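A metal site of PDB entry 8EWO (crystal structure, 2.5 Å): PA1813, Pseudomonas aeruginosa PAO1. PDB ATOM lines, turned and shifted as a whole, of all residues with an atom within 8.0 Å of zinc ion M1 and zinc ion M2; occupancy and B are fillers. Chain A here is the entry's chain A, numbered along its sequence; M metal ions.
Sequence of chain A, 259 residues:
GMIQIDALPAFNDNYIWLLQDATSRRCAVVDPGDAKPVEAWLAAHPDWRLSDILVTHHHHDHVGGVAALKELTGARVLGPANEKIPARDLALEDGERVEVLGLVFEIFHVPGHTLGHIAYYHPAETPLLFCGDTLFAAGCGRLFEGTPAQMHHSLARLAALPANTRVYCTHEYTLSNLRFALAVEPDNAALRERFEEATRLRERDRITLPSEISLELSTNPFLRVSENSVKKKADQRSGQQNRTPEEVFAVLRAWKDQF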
ATOM      1  N   ASP A  13     -17.412 -24.611 -12.539  1.00  0.00           N
ATOM      2  CA  ASP A  13     -16.800 -23.350 -12.151  1.00  0.00           C
ATOM      3  C   ASP A  13     -16.718 -23.174 -10.636  1.00  0.00           C
ATOM      4  O   ASP A  13     -16.599 -22.046 -10.153  1.00  0.00           O
ATOM      5  CB  ASP A  13     -17.576 -22.173 -12.759  1.00  0.00           C
ATOM      6  CG  ASP A  13     -19.074 -22.413 -12.774  1.00  0.00           C
ATOM      7  OD1 ASP A  13     -19.594 -23.059 -11.829  1.00  0.00           O
ATOM      8  OD2 ASP A  13     -19.747 -21.962 -13.726  1.00  0.00           O
ATOM      9  N   ASN A  14     -16.776 -24.265  -9.873  1.00  0.00           N
ATOM     10  CA  ASN A  14     -16.769 -24.186  -8.421  1.00  0.00           C
ATOM     11  C   ASN A  14     -15.347 -24.208  -7.884  1.00  0.00           C
ATOM     12  O   ASN A  14     -14.442 -24.819  -8.471  1.00  0.00           O
ATOM     13  CB  ASN A  14     -17.564 -25.352  -7.809  1.00  0.00           C
ATOM     14  CG  ASN A  14     -19.028 -25.014  -7.640  1.00  0.00           C
ATOM     15  OD1 ASN A  14     -19.484 -24.665  -6.548  1.00  0.00           O
ATOM     16  ND2 ASN A  14     -19.793 -25.117  -8.720  1.00  0.00           N
ATOM     17  N   ASP A  31     -17.436 -25.047   1.682  1.00  0.00           N
ATOM     18  CA  ASP A  31     -18.407 -25.490   0.684  1.00  0.00           C
ATOM     19  C   ASP A  31     -17.879 -26.622  -0.183  1.00  0.00           C
ATOM     20  O   ASP A  31     -17.660 -26.437  -1.386  1.00  0.00           O
ATOM     21  CB  ASP A  31     -18.823 -24.311  -0.197  1.00  0.00           C
ATOM     22  CG  ASP A  31     -19.693 -23.299   0.539  1.00  0.00           C
ATOM     23  OD1 ASP A  31     -20.375 -23.693   1.502  1.00  0.00           O
ATOM     24  OD2 ASP A  31     -19.688 -22.119   0.147  1.00  0.00           O
ATOM     25  N   THR A  56     -21.659 -22.200   3.508  1.00  0.00           N
ATOM     26  CA  THR A  56     -22.300 -20.891   3.384  1.00  0.00           C
ATOM     27  C   THR A  56     -23.810 -20.993   3.205  1.00  0.00           C
ATOM     28  O   THR A  56     -24.559 -20.350   3.952  1.00  0.00           O
ATOM     29  CB  THR A  56     -21.689 -20.105   2.223  1.00  0.00           C
ATOM     30  OG1 THR A  56     -21.902 -20.808   0.992  1.00  0.00           O
ATOM     31  CG2 THR A  56     -20.197 -19.905   2.442  1.00  0.00           C
ATOM     32  N   HIS A  57     -24.280 -21.777   2.233  1.00  0.00           N
ATOM     33  CA  HIS A  57     -25.713 -21.997   2.042  1.00  0.00           C
ATOM     34  C   HIS A  57     -25.949 -23.433   1.600  1.00  0.00           C
ATOM     35  O   HIS A  57     -25.011 -24.198   1.340  1.00  0.00           O
ATOM     36  CB  HIS A  57     -26.320 -20.993   1.050  1.00  0.00           C
ATOM     37  CG  HIS A  57     -25.755 -21.080  -0.342  1.00  0.00           C
ATOM     38  ND1 HIS A  57     -24.425 -20.863  -0.616  1.00  0.00           N
ATOM     39  CD2 HIS A  57     -26.349 -21.341  -1.525  1.00  0.00           C
ATOM     40  CE1 HIS A  57     -24.227 -20.996  -1.921  1.00  0.00           C
ATOM     41  NE2 HIS A  57     -25.371 -21.287  -2.486  1.00  0.00           N
ATOM     42  N   HIS A  58     -27.222 -23.796   1.502  1.00  0.00           N
ATOM     43  CA  HIS A  58     -27.666 -25.181   1.389  1.00  0.00           C
ATOM     44  C   HIS A  58     -27.618 -25.742  -0.036  1.00  0.00           C
ATOM     45  O   HIS A  58     -28.107 -26.855  -0.252  1.00  0.00           O
ATOM     46  CB  HIS A  58     -29.092 -25.320   1.932  1.00  0.00           C
ATOM     47  CG  HIS A  58     -30.129 -24.662   1.075  1.00  0.00           C
ATOM     48  ND1 HIS A  58     -30.917 -25.361   0.187  1.00  0.00           N
ATOM     49  CD2 HIS A  58     -30.506 -23.364   0.958  1.00  0.00           C
ATOM     50  CE1 HIS A  58     -31.732 -24.527  -0.431  1.00  0.00           C
ATOM     51  NE2 HIS A  58     -31.505 -23.305   0.020  1.00  0.00           N
ATOM     52  N   HIS A  59     -27.062 -25.012  -0.999  1.00  0.00           N
ATOM     53  CA  HIS A  59     -27.158 -25.446  -2.383  1.00  0.00           C
ATOM     54  C   HIS A  59     -26.282 -26.670  -2.646  1.00  0.00           C
ATOM     55  O   HIS A  59     -25.276 -26.898  -1.968  1.00  0.00           O
ATOM     56  CB  HIS A  59     -26.782 -24.308  -3.328  1.00  0.00           C
ATOM     57  CG  HIS A  59     -27.930 -23.408  -3.655  1.00  0.00           C
ATOM     58  ND1 HIS A  59     -27.797 -22.257  -4.395  1.00  0.00           N
ATOM     59  CD2 HIS A  59     -29.247 -23.494  -3.330  1.00  0.00           C
ATOM     60  CE1 HIS A  59     -28.977 -21.670  -4.520  1.00  0.00           C
ATOM     61  NE2 HIS A  59     -29.875 -22.399  -3.888  1.00  0.00           N
ATOM     62  N   HIS A  60     -26.688 -27.456  -3.649  1.00  0.00           N
ATOM     63  CA  HIS A  60     -26.080 -28.765  -3.884  1.00  0.00           C
ATOM     64  C   HIS A  60     -24.585 -28.652  -4.132  1.00  0.00           C
ATOM     65  O   HIS A  60     -23.805 -29.475  -3.634  1.00  0.00           O
ATOM     66  CB  HIS A  60     -26.759 -29.440  -5.076  1.00  0.00           C
ATOM     67  CG  HIS A  60     -26.432 -28.813  -6.396  1.00  0.00           C
ATOM     68  ND1 HIS A  60     -27.057 -27.666  -6.845  1.00  0.00           N
ATOM     69  CD2 HIS A  60     -25.521 -29.151  -7.330  1.00  0.00           C
ATOM     70  CE1 HIS A  60     -26.557 -27.335  -8.021  1.00  0.00           C
ATOM     71  NE2 HIS A  60     -25.618 -28.217  -8.346  1.00  0.00           N
ATOM     72  N   ASP A  61     -24.161 -27.654  -4.902  1.00  0.00           N
ATOM     73  CA  ASP A  61     -22.749 -27.539  -5.257  1.00  0.00           C
ATOM     74  C   ASP A  61     -21.887 -27.050  -4.096  1.00  0.00           C
ATOM     75  O   ASP A  61     -20.692 -26.786  -4.303  1.00  0.00           O
ATOM     76  CB  ASP A  61     -22.581 -26.612  -6.459  1.00  0.00           C
ATOM     77  CG  ASP A  61     -23.322 -25.305  -6.298  1.00  0.00           C
ATOM     78  OD1 ASP A  61     -24.528 -25.339  -5.958  1.00  0.00           O
ATOM     79  OD2 ASP A  61     -22.705 -24.240  -6.487  1.00  0.00           O
ATOM     80  N   HIS A  62     -22.451 -26.933  -2.894  1.00  0.00           N
ATOM     81  CA  HIS A  62     -21.709 -26.536  -1.713  1.00  0.00           C
ATOM     82  C   HIS A  62     -21.743 -27.562  -0.592  1.00  0.00           C
ATOM     83  O   HIS A  62     -20.864 -27.533   0.271  1.00  0.00           O
ATOM     84  CB  HIS A  62     -22.226 -25.201  -1.168  1.00  0.00           C
ATOM     85  CG  HIS A  62     -22.202 -24.092  -2.170  1.00  0.00           C
ATOM     86  ND1 HIS A  62     -21.283 -23.070  -2.120  1.00  0.00           N
ATOM     87  CD2 HIS A  62     -22.977 -23.847  -3.253  1.00  0.00           C
ATOM     88  CE1 HIS A  62     -21.487 -22.239  -3.134  1.00  0.00           C
ATOM     89  NE2 HIS A  62     -22.510 -22.689  -3.834  1.00  0.00           N
ATOM     90  N   HIS A 113     -29.305 -14.511  -2.050  1.00  0.00           N
ATOM     91  CA  HIS A 113     -29.189 -15.723  -2.862  1.00  0.00           C
ATOM     92  C   HIS A 113     -30.063 -16.828  -2.292  1.00  0.00           C
ATOM     93  O   HIS A 113     -30.848 -17.456  -3.014  1.00  0.00           O
ATOM     94  CB  HIS A 113     -27.721 -16.152  -2.925  1.00  0.00           C
ATOM     95  CG  HIS A 113     -27.479 -17.342  -3.796  1.00  0.00           C
ATOM     96  ND1 HIS A 113     -27.496 -17.281  -5.169  1.00  0.00           N
ATOM     97  CD2 HIS A 113     -27.180 -18.625  -3.483  1.00  0.00           C
ATOM     98  CE1 HIS A 113     -27.230 -18.473  -5.669  1.00  0.00           C
ATOM     99  NE2 HIS A 113     -27.035 -19.311  -4.664  1.00  0.00           N
ATOM    100  N   THR A 114     -29.943 -17.083  -0.989  1.00  0.00           N
ATOM    101  CA  THR A 114     -30.864 -17.913  -0.238  1.00  0.00           C
ATOM    102  C   THR A 114     -31.269 -17.148   1.020  1.00  0.00           C
ATOM    103  O   THR A 114     -30.661 -16.147   1.381  1.00  0.00           O
ATOM    104  CB  THR A 114     -30.252 -19.270   0.135  1.00  0.00           C
ATOM    105  OG1 THR A 114     -29.136 -19.077   1.008  1.00  0.00           O
ATOM    106  CG2 THR A 114     -29.807 -20.023  -1.116  1.00  0.00           C
ATOM    107  N   HIS A 117     -28.427 -17.799   3.832  1.00  0.00           N
ATOM    108  CA  HIS A 117     -27.025 -17.668   3.472  1.00  0.00           C
ATOM    109  C   HIS A 117     -26.243 -16.881   4.520  1.00  0.00           C
ATOM    110  O   HIS A 117     -26.713 -15.864   5.036  1.00  0.00           O
ATOM    111  CB  HIS A 117     -26.904 -16.975   2.106  1.00  0.00           C
ATOM    112  CG  HIS A 117     -25.601 -17.215   1.406  1.00  0.00           C
ATOM    113  ND1 HIS A 117     -24.385 -16.975   1.990  1.00  0.00           N
ATOM    114  CD2 HIS A 117     -25.340 -17.652   0.152  1.00  0.00           C
ATOM    115  CE1 HIS A 117     -23.416 -17.267   1.136  1.00  0.00           C
ATOM    116  NE2 HIS A 117     -23.975 -17.677   0.014  1.00  0.00           N
ATOM    117  N   GLY A 132     -19.398 -17.165  -0.260  1.00  0.00           N
ATOM    118  CA  GLY A 132     -20.156 -18.167  -1.013  1.00  0.00           C
ATOM    119  C   GLY A 132     -20.692 -17.625  -2.322  1.00  0.00           C
ATOM    120  O   GLY A 132     -19.934 -17.256  -3.234  1.00  0.00           O
ATOM    121  N   ASP A 133     -22.024 -17.586  -2.431  1.00  0.00           N
ATOM    122  CA  ASP A 133     -22.704 -17.135  -3.647  1.00  0.00           C
ATOM    123  C   ASP A 133     -23.361 -15.770  -3.484  1.00  0.00           C
ATOM    124  O   ASP A 133     -24.151 -15.373  -4.344  1.00  0.00           O
ATOM    125  CB  ASP A 133     -23.759 -18.156  -4.068  1.00  0.00           C
ATOM    126  CG  ASP A 133     -23.153 -19.383  -4.712  1.00  0.00           C
ATOM    127  OD1 ASP A 133     -21.904 -19.468  -4.779  1.00  0.00           O
ATOM    128  OD2 ASP A 133     -23.912 -20.261  -5.170  1.00  0.00           O
ATOM    129  N   THR A 134     -23.067 -15.050  -2.396  1.00  0.00           N
ATOM    130  CA  THR A 134     -23.688 -13.746  -2.190  1.00  0.00           C
ATOM    131  C   THR A 134     -22.999 -12.670  -3.037  1.00  0.00           C
ATOM    132  O   THR A 134     -23.605 -12.111  -3.951  1.00  0.00           O
ATOM    133  CB  THR A 134     -23.660 -13.371  -0.701  1.00  0.00           C
ATOM    134  OG1 THR A 134     -24.401 -14.344   0.047  1.00  0.00           O
ATOM    135  CG2 THR A 134     -24.267 -11.995  -0.478  1.00  0.00           C
ATOM    136  N   PHE A 136     -19.997 -11.869  -5.684  1.00  0.00           N
ATOM    137  CA  PHE A 136     -19.072 -12.437  -6.655  1.00  0.00           C
ATOM    138  C   PHE A 136     -18.082 -11.375  -7.114  1.00  0.00           C
ATOM    139  O   PHE A 136     -18.269 -10.175  -6.880  1.00  0.00           O
ATOM    140  CB  PHE A 136     -19.831 -13.016  -7.859  1.00  0.00           C
ATOM    141  CG  PHE A 136     -20.479 -14.339  -7.582  1.00  0.00           C
ATOM    142  CD1 PHE A 136     -19.779 -15.357  -6.976  1.00  0.00           C
ATOM    143  CD2 PHE A 136     -21.795 -14.562  -7.961  1.00  0.00           C
ATOM    144  CE1 PHE A 136     -20.378 -16.582  -6.732  1.00  0.00           C
ATOM    145  CE2 PHE A 136     -22.398 -15.778  -7.720  1.00  0.00           C
ATOM    146  CZ  PHE A 136     -21.690 -16.789  -7.106  1.00  0.00           C
ATOM    147  N   GLY A 141     -24.929 -13.057  -6.619  1.00  0.00           N
ATOM    148  CA  GLY A 141     -25.717 -14.240  -6.888  1.00  0.00           C
ATOM    149  C   GLY A 141     -27.123 -13.919  -7.337  1.00  0.00           C
ATOM    150  O   GLY A 141     -27.645 -12.824  -7.133  1.00  0.00           O
ATOM    151  N   ARG A 142     -27.756 -14.908  -7.966  1.00  0.00           N
ATOM    152  CA  ARG A 142     -29.135 -14.775  -8.382  1.00  0.00           C
ATOM    153  C   ARG A 142     -30.056 -14.941  -7.182  1.00  0.00           C
ATOM    154  O   ARG A 142     -29.736 -15.629  -6.205  1.00  0.00           O
ATOM    155  CB  ARG A 142     -29.487 -15.816  -9.457  1.00  0.00           C
ATOM    156  CG  ARG A 142     -28.686 -15.659 -10.740  1.00  0.00           C
ATOM    157  CD  ARG A 142     -28.936 -16.824 -11.676  1.00  0.00           C
ATOM    158  NE  ARG A 142     -30.277 -16.795 -12.246  1.00  0.00           N
ATOM    159  CZ  ARG A 142     -30.578 -16.340 -13.450  1.00  0.00           C
ATOM    160  NH1 ARG A 142     -29.651 -15.873 -14.267  1.00  0.00           N
ATOM    161  NH2 ARG A 142     -31.845 -16.368 -13.853  1.00  0.00           N
ATOM    162  N   PHE A 144     -32.456 -16.657  -5.846  1.00  0.00           N
ATOM    163  CA  PHE A 144     -33.196 -17.912  -5.815  1.00  0.00           C
ATOM    164  C   PHE A 144     -34.287 -17.886  -4.755  1.00  0.00           C
ATOM    165  O   PHE A 144     -35.357 -18.476  -4.964  1.00  0.00           O
ATOM    166  CB  PHE A 144     -32.248 -19.080  -5.578  1.00  0.00           C
ATOM    167  CG  PHE A 144     -31.540 -19.558  -6.814  1.00  0.00           C
ATOM    168  CD1 PHE A 144     -32.211 -20.274  -7.791  1.00  0.00           C
ATOM    169  CD2 PHE A 144     -30.188 -19.306  -6.984  1.00  0.00           C
ATOM    170  CE1 PHE A 144     -31.553 -20.708  -8.926  1.00  0.00           C
ATOM    171  CE2 PHE A 144     -29.521 -19.736  -8.121  1.00  0.00           C
ATOM    172  CZ  PHE A 144     -30.206 -20.444  -9.090  1.00  0.00           C
ATOM    173  N   THR A 170     -17.347 -18.343  -4.448  1.00  0.00           N
ATOM    174  CA  THR A 170     -17.257 -19.753  -4.801  1.00  0.00           C
ATOM    175  C   THR A 170     -16.990 -19.993  -6.281  1.00  0.00           C
ATOM    176  O   THR A 170     -16.208 -20.882  -6.627  1.00  0.00           O
ATOM    177  CB  THR A 170     -18.551 -20.475  -4.397  1.00  0.00           C
ATOM    178  OG1 THR A 170     -18.822 -20.234  -3.013  1.00  0.00           O
ATOM    179  CG2 THR A 170     -18.426 -21.972  -4.646  1.00  0.00           C
ATOM    180  N   HIS A 171     -17.606 -19.217  -7.164  1.00  0.00           N
ATOM    181  CA  HIS A 171     -17.675 -19.574  -8.574  1.00  0.00           C
ATOM    182  C   HIS A 171     -16.731 -18.731  -9.424  1.00  0.00           C
ATOM    183  O   HIS A 171     -16.423 -17.583  -9.105  1.00  0.00           O
ATOM    184  CB  HIS A 171     -19.103 -19.423  -9.103  1.00  0.00           C
ATOM    185  CG  HIS A 171     -20.067 -20.412  -8.541  1.00  0.00           C
ATOM    186  ND1 HIS A 171     -20.239 -21.676  -9.063  1.00  0.00           N
ATOM    187  CD2 HIS A 171     -20.929 -20.326  -7.489  1.00  0.00           C
ATOM    188  CE1 HIS A 171     -21.156 -22.321  -8.364  1.00  0.00           C
ATOM    189  NE2 HIS A 171     -21.590 -21.521  -7.405  1.00  0.00           N
ATOM    190  N   TYR A 173     -17.041 -16.900 -12.037  1.00  0.00           N
ATOM    191  CA  TYR A 173     -17.975 -16.107 -12.833  1.00  0.00           C
ATOM    192  C   TYR A 173     -17.393 -14.779 -13.302  1.00  0.00           C
ATOM    193  O   TYR A 173     -18.119 -13.984 -13.896  1.00  0.00           O
ATOM    194  CB  TYR A 173     -19.252 -15.840 -12.026  1.00  0.00           C
ATOM    195  CG  TYR A 173     -20.142 -17.039 -11.773  1.00  0.00           C
ATOM    196  CD1 TYR A 173     -20.102 -18.143 -12.601  1.00  0.00           C
ATOM    197  CD2 TYR A 173     -21.058 -17.031 -10.726  1.00  0.00           C
ATOM    198  CE1 TYR A 173     -20.921 -19.240 -12.371  1.00  0.00           C
ATOM    199  CE2 TYR A 173     -21.881 -18.117 -10.490  1.00  0.00           C
ATOM    200  CZ  TYR A 173     -21.810 -19.213 -11.310  1.00  0.00           C
ATOM    201  OH  TYR A 173     -22.637 -20.294 -11.085  1.00  0.00           O
HETATM  202 ZN    ZN M   1     -25.788 -21.227  -4.655  1.00  0.00          ZN
HETATM  203 ZN    ZN M   2     -23.250 -22.140  -5.939  1.00  0.00          ZN
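Zinc ion M1 is bound by the side-chain carboxylate (OD2) of Asp 133 (2.2 Å).
A ring nitrogen (NE2) of His 57 binds zinc ion M1 (2.2 Å).
A ring nitrogen (ND1) of His 59 is bound to zinc ion M1 (2.3 Å).
A ring nitrogen (NE2) of His 113 binds zinc ion M1 (2.3 Å).
The backbone NH of Asp 133 lies within hydrogen-bond range of a ring nitrogen (NE2) of His 117 (3.1 Å).
A ring nitrogen (NE2) of His 117 lies within hydrogen-bond range of a ring nitrogen (ND1) of His 57.
The side-chain hydroxyl of Thr 56 lies within hydrogen-bond range of a ring nitrogen (ND1) of His 57 (3.0 Å).
The side-chain amide oxygen (OD1) of Asn 14 lies close to the backbone carbonyl oxygen (O) of Asp 61, 3.3 Å away.
The backbone carbonyl oxygen of His 113 sits close to the backbone NH of Phe 144 (3.4 Å).
A ring nitrogen (ND1) of His 62 is in hydrogen-bond range of the side-chain carboxylate (OD2) of Asp 31, 2.9 Å away.
ND1 of His 171 sits close to ND2 of Asn 14, at 3.5 Å.
OD1 of Asp 13 lies within hydrogen-bond range of ND1 of His 171.
Four residues have an atom within 4 Å of zinc ion M2: Asp 61, His 62, Asp 133 and His 171.
The nearest printed residue that does not touch zinc ion M2 is His 57 (4.1 Å).
Zinc ion M2 is bound by OD2 of Asp 133 (2.1 Å), OD2 of Asp 61 (2.2 Å), NE2 of His 62 (2.3 Å) and NE2 of His 171 (2.3 Å).
Five residues have an atom within 4 Å of zinc ion M1: His 57, His 59, His 62, His 113 and Asp 133.
The nearest printed residue that does not touch zinc ion M1 is Asp 61 (4.5 Å).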
